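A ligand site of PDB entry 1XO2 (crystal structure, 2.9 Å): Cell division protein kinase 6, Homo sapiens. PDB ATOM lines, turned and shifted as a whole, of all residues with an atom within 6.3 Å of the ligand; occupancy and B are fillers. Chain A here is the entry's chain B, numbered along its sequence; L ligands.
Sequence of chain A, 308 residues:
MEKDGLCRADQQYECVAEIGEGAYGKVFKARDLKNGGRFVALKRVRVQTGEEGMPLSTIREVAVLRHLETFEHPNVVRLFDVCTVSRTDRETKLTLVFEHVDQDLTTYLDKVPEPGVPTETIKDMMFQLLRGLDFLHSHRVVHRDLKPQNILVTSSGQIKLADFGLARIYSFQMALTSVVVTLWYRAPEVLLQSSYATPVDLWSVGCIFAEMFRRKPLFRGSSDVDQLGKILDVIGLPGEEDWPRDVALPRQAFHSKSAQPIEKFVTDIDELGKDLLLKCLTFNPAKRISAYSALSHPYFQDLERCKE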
ATOM      1  N   ILE A  19       0.797 -10.847  20.290  1.00  0.00           N
ATOM      2  CA  ILE A  19       1.268 -11.610  19.138  1.00  0.00           C
ATOM      3  C   ILE A  19       0.160 -12.528  18.682  1.00  0.00           C
ATOM      4  O   ILE A  19       0.363 -13.707  18.391  1.00  0.00           O
ATOM      5  CB  ILE A  19       2.543 -12.426  19.469  1.00  0.00           C
ATOM      6  CG1 ILE A  19       2.328 -13.297  20.700  1.00  0.00           C
ATOM      7  CG2 ILE A  19       3.713 -11.479  19.694  1.00  0.00           C
ATOM      8  CD1 ILE A  19       3.573 -14.057  21.122  1.00  0.00           C
ATOM      9  N   GLY A  20      -1.035 -11.960  18.616  1.00  0.00           N
ATOM     10  CA  GLY A  20      -2.197 -12.735  18.223  1.00  0.00           C
ATOM     11  C   GLY A  20      -2.976 -13.105  19.464  1.00  0.00           C
ATOM     12  O   GLY A  20      -2.402 -13.339  20.531  1.00  0.00           O
ATOM     13  N   GLY A  22      -6.020 -15.621  21.227  1.00  0.00           N
ATOM     14  CA  GLY A  22      -6.809 -16.822  21.080  1.00  0.00           C
ATOM     15  C   GLY A  22      -8.280 -16.460  21.126  1.00  0.00           C
ATOM     16  O   GLY A  22      -8.685 -15.406  20.617  1.00  0.00           O
ATOM     17  N   VAL A  27      -2.614 -13.218  23.506  1.00  0.00           N
ATOM     18  CA  VAL A  27      -1.295 -13.762  23.792  1.00  0.00           C
ATOM     19  C   VAL A  27      -0.235 -12.684  23.573  1.00  0.00           C
ATOM     20  O   VAL A  27       0.176 -12.432  22.440  1.00  0.00           O
ATOM     21  CB  VAL A  27      -1.004 -14.963  22.895  1.00  0.00           C
ATOM     22  CG1 VAL A  27       0.344 -15.543  23.229  1.00  0.00           C
ATOM     23  CG2 VAL A  27      -2.084 -16.012  23.071  1.00  0.00           C
ATOM     24  N   ALA A  41       6.432 -16.053  26.288  1.00  0.00           N
ATOM     25  CA  ALA A  41       5.084 -15.877  25.738  1.00  0.00           C
ATOM     26  C   ALA A  41       4.082 -15.901  26.882  1.00  0.00           C
ATOM     27  O   ALA A  41       4.127 -16.803  27.725  1.00  0.00           O
ATOM     28  CB  ALA A  41       4.777 -16.980  24.756  1.00  0.00           C
ATOM     29  N   LEU A  42       3.196 -14.911  26.937  1.00  0.00           N
ATOM     30  CA  LEU A  42       2.189 -14.832  27.987  1.00  0.00           C
ATOM     31  C   LEU A  42       0.775 -15.066  27.514  1.00  0.00           C
ATOM     32  O   LEU A  42       0.203 -14.260  26.779  1.00  0.00           O
ATOM     33  CB  LEU A  42       2.216 -13.476  28.686  1.00  0.00           C
ATOM     34  CG  LEU A  42       3.299 -13.213  29.720  1.00  0.00           C
ATOM     35  CD1 LEU A  42       2.706 -12.306  30.783  1.00  0.00           C
ATOM     36  CD2 LEU A  42       3.758 -14.503  30.354  1.00  0.00           C
ATOM     37  N   LYS A  43       0.188 -16.161  27.971  1.00  0.00           N
ATOM     38  CA  LYS A  43      -1.169 -16.490  27.618  1.00  0.00           C
ATOM     39  C   LYS A  43      -2.009 -16.348  28.870  1.00  0.00           C
ATOM     40  O   LYS A  43      -2.131 -17.279  29.652  1.00  0.00           O
ATOM     41  CB  LYS A  43      -1.245 -17.920  27.094  1.00  0.00           C
ATOM     42  CG  LYS A  43      -2.577 -18.281  26.493  1.00  0.00           C
ATOM     43  CD  LYS A  43      -2.580 -19.704  25.978  1.00  0.00           C
ATOM     44  CE  LYS A  43      -3.911 -20.023  25.334  1.00  0.00           C
ATOM     45  NZ  LYS A  43      -3.970 -21.404  24.828  1.00  0.00           N
ATOM     46  N   GLU A  61      -4.742 -28.215  28.732  1.00  0.00           N
ATOM     47  CA  GLU A  61      -3.473 -27.807  28.166  1.00  0.00           C
ATOM     48  C   GLU A  61      -2.287 -27.998  29.122  1.00  0.00           C
ATOM     49  O   GLU A  61      -1.384 -28.817  28.869  1.00  0.00           O
ATOM     50  CB  GLU A  61      -3.534 -26.338  27.705  1.00  0.00           C
ATOM     51  CG  GLU A  61      -2.219 -25.798  27.197  1.00  0.00           C
ATOM     52  CD  GLU A  61      -2.382 -24.565  26.344  1.00  0.00           C
ATOM     53  OE1 GLU A  61      -3.217 -23.713  26.698  1.00  0.00           O
ATOM     54  OE2 GLU A  61      -1.668 -24.459  25.334  1.00  0.00           O
ATOM     55  N   LEU A  65       0.779 -30.706  28.530  1.00  0.00           N
ATOM     56  CA  LEU A  65       2.149 -30.229  28.431  1.00  0.00           C
ATOM     57  C   LEU A  65       2.948 -30.701  29.642  1.00  0.00           C
ATOM     58  O   LEU A  65       3.958 -31.407  29.487  1.00  0.00           O
ATOM     59  CB  LEU A  65       2.160 -28.713  28.306  1.00  0.00           C
ATOM     60  CG  LEU A  65       1.652 -28.260  26.925  1.00  0.00           C
ATOM     61  CD1 LEU A  65       1.171 -26.806  26.940  1.00  0.00           C
ATOM     62  CD2 LEU A  65       2.770 -28.456  25.908  1.00  0.00           C
ATOM     63  N   VAL A  77       6.263 -27.006  22.117  1.00  0.00           N
ATOM     64  CA  VAL A  77       6.600 -25.772  22.825  1.00  0.00           C
ATOM     65  C   VAL A  77       6.733 -25.994  24.325  1.00  0.00           C
ATOM     66  O   VAL A  77       6.139 -26.907  24.883  1.00  0.00           O
ATOM     67  CB  VAL A  77       5.549 -24.656  22.567  1.00  0.00           C
ATOM     68  CG1 VAL A  77       4.174 -25.091  23.075  1.00  0.00           C
ATOM     69  CG2 VAL A  77       6.009 -23.372  23.231  1.00  0.00           C
ATOM     70  N   LEU A  96      -0.773 -17.768  32.023  1.00  0.00           N
ATOM     71  CA  LEU A  96       0.064 -18.918  31.691  1.00  0.00           C
ATOM     72  C   LEU A  96       1.287 -18.370  30.925  1.00  0.00           C
ATOM     73  O   LEU A  96       1.138 -17.633  29.936  1.00  0.00           O
ATOM     74  CB  LEU A  96      -0.757 -19.869  30.803  1.00  0.00           C
ATOM     75  CG  LEU A  96      -0.774 -21.388  31.021  1.00  0.00           C
ATOM     76  CD1 LEU A  96      -1.125 -21.707  32.464  1.00  0.00           C
ATOM     77  CD2 LEU A  96      -1.798 -22.017  30.071  1.00  0.00           C
ATOM     78  N   PHE A  98       4.592 -19.120  28.669  1.00  0.00           N
ATOM     79  CA  PHE A  98       5.313 -20.062  27.827  1.00  0.00           C
ATOM     80  C   PHE A  98       6.663 -19.495  27.359  1.00  0.00           C
ATOM     81  O   PHE A  98       7.091 -18.421  27.783  1.00  0.00           O
ATOM     82  CB  PHE A  98       4.493 -20.413  26.583  1.00  0.00           C
ATOM     83  CG  PHE A  98       3.193 -21.096  26.874  1.00  0.00           C
ATOM     84  CD1 PHE A  98       2.132 -20.388  27.414  1.00  0.00           C
ATOM     85  CD2 PHE A  98       3.016 -22.433  26.544  1.00  0.00           C
ATOM     86  CE1 PHE A  98       0.885 -20.994  27.602  1.00  0.00           C
ATOM     87  CE2 PHE A  98       1.788 -23.055  26.731  1.00  0.00           C
ATOM     88  CZ  PHE A  98       0.718 -22.332  27.270  1.00  0.00           C
ATOM     89  N   GLU A  99       7.322 -20.226  26.465  1.00  0.00           N
ATOM     90  CA  GLU A  99       8.588 -19.760  25.926  1.00  0.00           C
ATOM     91  C   GLU A  99       8.197 -18.922  24.720  1.00  0.00           C
ATOM     92  O   GLU A  99       7.107 -19.091  24.173  1.00  0.00           O
ATOM     93  CB  GLU A  99       9.488 -20.927  25.485  1.00  0.00           C
ATOM     94  CG  GLU A  99       9.001 -21.686  24.256  1.00  0.00           C
ATOM     95  CD  GLU A  99      10.047 -22.622  23.666  1.00  0.00           C
ATOM     96  OE1 GLU A  99      11.088 -22.119  23.180  1.00  0.00           O
ATOM     97  OE2 GLU A  99       9.847 -23.860  23.688  1.00  0.00           O
ATOM     98  N   HIS A 100       9.080 -18.011  24.310  1.00  0.00           N
ATOM     99  CA  HIS A 100       8.781 -17.187  23.149  1.00  0.00           C
ATOM    100  C   HIS A 100       9.677 -17.502  21.970  1.00  0.00           C
ATOM    101  O   HIS A 100      10.894 -17.452  22.068  1.00  0.00           O
ATOM    102  CB  HIS A 100       8.911 -15.711  23.472  1.00  0.00           C
ATOM    103  CG  HIS A 100       8.676 -14.830  22.285  1.00  0.00           C
ATOM    104  ND1 HIS A 100       9.616 -13.933  21.823  1.00  0.00           N
ATOM    105  CD2 HIS A 100       7.609 -14.719  21.453  1.00  0.00           C
ATOM    106  CE1 HIS A 100       9.140 -13.310  20.754  1.00  0.00           C
ATOM    107  NE2 HIS A 100       7.926 -13.770  20.504  1.00  0.00           N
ATOM    108  N   VAL A 101       9.046 -17.839  20.858  1.00  0.00           N
ATOM    109  CA  VAL A 101       9.750 -18.144  19.639  1.00  0.00           C
ATOM    110  C   VAL A 101       9.673 -16.855  18.802  1.00  0.00           C
ATOM    111  O   VAL A 101       8.810 -16.026  19.037  1.00  0.00           O
ATOM    112  CB  VAL A 101       9.087 -19.318  18.919  1.00  0.00           C
ATOM    113  CG1 VAL A 101       9.810 -19.612  17.642  1.00  0.00           C
ATOM    114  CG2 VAL A 101       9.104 -20.535  19.821  1.00  0.00           C
ATOM    115  N   ASP A 102      10.575 -16.702  17.829  1.00  0.00           N
ATOM    116  CA  ASP A 102      10.622 -15.495  17.016  1.00  0.00           C
ATOM    117  C   ASP A 102       9.334 -15.125  16.266  1.00  0.00           C
ATOM    118  O   ASP A 102       9.056 -13.947  16.058  1.00  0.00           O
ATOM    119  CB  ASP A 102      11.802 -15.589  16.043  1.00  0.00           C
ATOM    120  CG  ASP A 102      13.130 -15.751  16.771  1.00  0.00           C
ATOM    121  OD1 ASP A 102      13.498 -14.859  17.557  1.00  0.00           O
ATOM    122  OD2 ASP A 102      13.804 -16.775  16.550  1.00  0.00           O
ATOM    123  N   GLN A 103       8.561 -16.123  15.844  1.00  0.00           N
ATOM    124  CA  GLN A 103       7.312 -15.877  15.117  1.00  0.00           C
ATOM    125  C   GLN A 103       6.558 -17.164  14.822  1.00  0.00           C
ATOM    126  O   GLN A 103       7.118 -18.254  14.878  1.00  0.00           O
ATOM    127  CB  GLN A 103       7.591 -15.128  13.800  1.00  0.00           C
ATOM    128  CG  GLN A 103       9.056 -15.048  13.375  1.00  0.00           C
ATOM    129  CD  GLN A 103       9.379 -15.843  12.118  1.00  0.00           C
ATOM    130  OE1 GLN A 103      10.546 -15.953  11.720  1.00  0.00           O
ATOM    131  NE2 GLN A 103       8.358 -16.391  11.477  1.00  0.00           N
ATOM    132  N   ASP A 104       5.268 -17.036  14.532  1.00  0.00           N
ATOM    133  CA  ASP A 104       4.483 -18.214  14.201  1.00  0.00           C
ATOM    134  C   ASP A 104       4.756 -18.493  12.742  1.00  0.00           C
ATOM    135  O   ASP A 104       5.491 -17.745  12.102  1.00  0.00           O
ATOM    136  CB  ASP A 104       2.991 -17.944  14.420  1.00  0.00           C
ATOM    137  CG  ASP A 104       2.493 -16.710  13.705  1.00  0.00           C
ATOM    138  OD1 ASP A 104       3.090 -15.631  13.893  1.00  0.00           O
ATOM    139  OD2 ASP A 104       1.509 -16.817  12.945  1.00  0.00           O
ATOM    140  N   THR A 107       3.282 -15.914  10.009  1.00  0.00           N
ATOM    141  CA  THR A 107       4.146 -14.735   9.905  1.00  0.00           C
ATOM    142  C   THR A 107       5.351 -15.021   9.013  1.00  0.00           C
ATOM    143  O   THR A 107       5.786 -14.185   8.225  1.00  0.00           O
ATOM    144  CB  THR A 107       4.640 -14.298  11.298  1.00  0.00           C
ATOM    145  OG1 THR A 107       3.582 -13.649  12.002  1.00  0.00           O
ATOM    146  CG2 THR A 107       5.853 -13.359  11.188  1.00  0.00           C
ATOM    147  N   GLN A 149      -1.095 -20.551  12.606  1.00  0.00           N
ATOM    148  CA  GLN A 149      -1.042 -19.674  13.777  1.00  0.00           C
ATOM    149  C   GLN A 149      -0.587 -20.396  15.027  1.00  0.00           C
ATOM    150  O   GLN A 149      -0.059 -19.778  15.946  1.00  0.00           O
ATOM    151  CB  GLN A 149      -2.394 -19.010  14.015  1.00  0.00           C
ATOM    152  CG  GLN A 149      -2.523 -18.224  15.340  1.00  0.00           C
ATOM    153  CD  GLN A 149      -1.545 -17.041  15.491  1.00  0.00           C
ATOM    154  OE1 GLN A 149      -1.963 -15.931  15.845  1.00  0.00           O
ATOM    155  NE2 GLN A 149      -0.263 -17.286  15.246  1.00  0.00           N
ATOM    156  N   ASN A 150      -0.763 -21.713  15.085  1.00  0.00           N
ATOM    157  CA  ASN A 150      -0.346 -22.463  16.251  1.00  0.00           C
ATOM    158  C   ASN A 150       1.043 -23.125  16.140  1.00  0.00           C
ATOM    159  O   ASN A 150       1.460 -23.841  17.036  1.00  0.00           O
ATOM    160  CB  ASN A 150      -1.413 -23.492  16.639  1.00  0.00           C
ATOM    161  CG  ASN A 150      -2.690 -22.841  17.185  1.00  0.00           C
ATOM    162  OD1 ASN A 150      -2.625 -22.036  18.123  1.00  0.00           O
ATOM    163  ND2 ASN A 150      -3.838 -23.176  16.602  1.00  0.00           N
ATOM    164  N   LEU A 152       5.067 -22.555  16.048  1.00  0.00           N
ATOM    165  CA  LEU A 152       6.103 -21.559  16.301  1.00  0.00           C
ATOM    166  C   LEU A 152       7.380 -21.870  15.498  1.00  0.00           C
ATOM    167  O   LEU A 152       7.932 -22.972  15.598  1.00  0.00           O
ATOM    168  CB  LEU A 152       6.443 -21.509  17.790  1.00  0.00           C
ATOM    169  CG  LEU A 152       5.257 -21.365  18.741  1.00  0.00           C
ATOM    170  CD1 LEU A 152       5.775 -20.981  20.113  1.00  0.00           C
ATOM    171  CD2 LEU A 152       4.296 -20.316  18.204  1.00  0.00           C
ATOM    172  N   ALA A 162       2.161 -25.503  19.211  1.00  0.00           N
ATOM    173  CA  ALA A 162       1.631 -24.679  20.294  1.00  0.00           C
ATOM    174  C   ALA A 162       0.108 -24.685  20.430  1.00  0.00           C
ATOM    175  O   ALA A 162      -0.611 -25.239  19.590  1.00  0.00           O
ATOM    176  CB  ALA A 162       2.125 -23.246  20.124  1.00  0.00           C
ATOM    177  N   ASP A 163      -0.393 -24.077  21.503  1.00  0.00           N
ATOM    178  CA  ASP A 163      -1.829 -23.987  21.774  1.00  0.00           C
ATOM    179  C   ASP A 163      -2.510 -25.347  21.881  1.00  0.00           C
ATOM    180  O   ASP A 163      -3.220 -25.776  20.980  1.00  0.00           O
ATOM    181  CB  ASP A 163      -2.508 -23.168  20.676  1.00  0.00           C
ATOM    182  CG  ASP A 163      -3.847 -22.585  21.127  1.00  0.00           C
ATOM    183  OD1 ASP A 163      -4.713 -23.347  21.596  1.00  0.00           O
ATOM    184  OD2 ASP A 163      -4.026 -21.356  20.998  1.00  0.00           O
ATOM    185  N   PHE A 164      -2.278 -26.016  23.006  1.00  0.00           N
ATOM    186  CA  PHE A 164      -2.875 -27.316  23.241  1.00  0.00           C
ATOM    187  C   PHE A 164      -4.235 -27.158  23.910  1.00  0.00           C
ATOM    188  O   PHE A 164      -4.768 -28.089  24.522  1.00  0.00           O
ATOM    189  CB  PHE A 164      -1.949 -28.173  24.122  1.00  0.00           C
ATOM    190  CG  PHE A 164      -0.764 -28.744  23.388  1.00  0.00           C
ATOM    191  CD1 PHE A 164      -0.668 -30.117  23.157  1.00  0.00           C
ATOM    192  CD2 PHE A 164       0.258 -27.912  22.895  1.00  0.00           C
ATOM    193  CE1 PHE A 164       0.441 -30.665  22.455  1.00  0.00           C
ATOM    194  CE2 PHE A 164       1.358 -28.445  22.192  1.00  0.00           C
ATOM    195  CZ  PHE A 164       1.445 -29.817  21.976  1.00  0.00           C
ATOM    196  N   GLY A 165      -4.820 -25.969  23.768  1.00  0.00           N
ATOM    197  CA  GLY A 165      -6.112 -25.698  24.367  1.00  0.00           C
ATOM    198  C   GLY A 165      -7.161 -26.782  24.209  1.00  0.00           C
ATOM    199  O   GLY A 165      -7.973 -27.003  25.108  1.00  0.00           O
HETATM  200  C1  LIG L   1       3.587 -15.586  17.323  1.00  0.00           C
HETATM  201  C2  LIG L   1       4.428 -16.139  18.335  1.00  0.00           C
HETATM  202  C3  LIG L   1       3.897 -17.078  19.407  1.00  0.00           C
HETATM  203  C4  LIG L   1       2.453 -17.370  19.264  1.00  0.00           C
HETATM  204  C5  LIG L   1       1.612 -16.803  18.223  1.00  0.00           C
HETATM  205  C6  LIG L   1       2.177 -15.879  17.263  1.00  0.00           C
HETATM  206  C7  LIG L   1       4.670 -17.671  20.530  1.00  0.00           C
HETATM  207  C8  LIG L   1       3.939 -18.557  21.520  1.00  0.00           C
HETATM  208  C9  LIG L   1       2.535 -18.847  21.367  1.00  0.00           C
HETATM  209  C10 LIG L   1       1.606 -19.686  22.132  1.00  0.00           C
HETATM  210  C11 LIG L   1       2.045 -20.556  23.159  1.00  0.00           C
HETATM  211  C12 LIG L   1       1.127 -21.362  23.873  1.00  0.00           C
HETATM  212  C13 LIG L   1      -0.251 -21.297  23.561  1.00  0.00           C
HETATM  213  C14 LIG L   1      -0.759 -20.433  22.566  1.00  0.00           C
HETATM  214  C15 LIG L   1       0.138 -19.632  21.846  1.00  0.00           C
HETATM  215  O1  LIG L   1       1.862 -18.263  20.253  1.00  0.00           O
HETATM  216  O2  LIG L   1       5.918 -17.457  20.728  1.00  0.00           O
HETATM  217  O3  LIG L   1      -2.142 -20.478  22.356  1.00  0.00           O
HETATM  218  O4  LIG L   1      -1.077 -22.083  24.269  1.00  0.00           O
HETATM  219  O5  LIG L   1       4.652 -19.118  22.602  1.00  0.00           O
HETATM  220  O6  LIG L   1       1.343 -15.281  16.306  1.00  0.00           O
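O2 of the ligand is in hydrogen-bond range of N of Val 101, 3.2 Å away. The backbone NH (N) of Asp 163 sits close to an oxygen (O4) of the ligand (3.5 Å). The side-chain carboxylate of Asp 163 lies within hydrogen-bond range of an oxygen (O3) of the ligand (2.5 Å). An oxygen (O5) of the ligand sits at hydrogen-bond distance from the backbone carbonyl oxygen (O) of Glu 99 (2.9 Å). OE2 of Glu 61 lies within hydrogen-bond range of O4 of the ligand (2.7 Å). O of Ile 19 sits at hydrogen-bond distance from O6 of the ligand, 2.8 Å away. An oxygen (O4) of the ligand lies within hydrogen-bond range of the side-chain amino group (NZ) of Lys 43 (3.0 Å). NE2 of Gln 149 lies within hydrogen-bond range of O6 of the ligand, 2.8 Å away. OD1 of Asp 104 sits at hydrogen-bond distance from O6 of the ligand, 3.0 Å away.
OG1 of Thr 107 is in hydrogen-bond range of OD1 of Asp 104, at 2.8 Å. The side-chain carboxylate of Glu 61 is in hydrogen-bond range of the backbone NH of Phe 164 (2.9 Å). The side-chain amino group (NZ) of Lys 43 is in salt-bridge range of the side-chain carboxylate (OE1) of Glu 61 (3.1 Å). OD2 of Asp 163 sits close to OD1 of Asn 150 (3.3 Å). O of Val 27 is in hydrogen-bond range of N of Ile 19 (2.7 Å). The side-chain carboxylate (OD2) of Asp 163 is in salt-bridge range of the side-chain amino group (NZ) of Lys 43 (3.8 Å). The backbone carbonyl oxygen (O) of Ala 41 is in hydrogen-bond range of the backbone NH (N) of Phe 98 (2.5 Å). The side-chain carboxylate (OD2) of Asp 104 sits at hydrogen-bond distance from the side-chain amide nitrogen (NE2) of Gln 149, at 2.9 Å.
Ala 41 touches the ligand. Phe 98 touches the ligand. His 100 touches the ligand (CD2 to O2, 3.3 Å). CD1 of Leu 152 touches O5 of the ligand (3.3 Å). Of the 26 residues printed, 12 come within 4 Å of the ligand.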
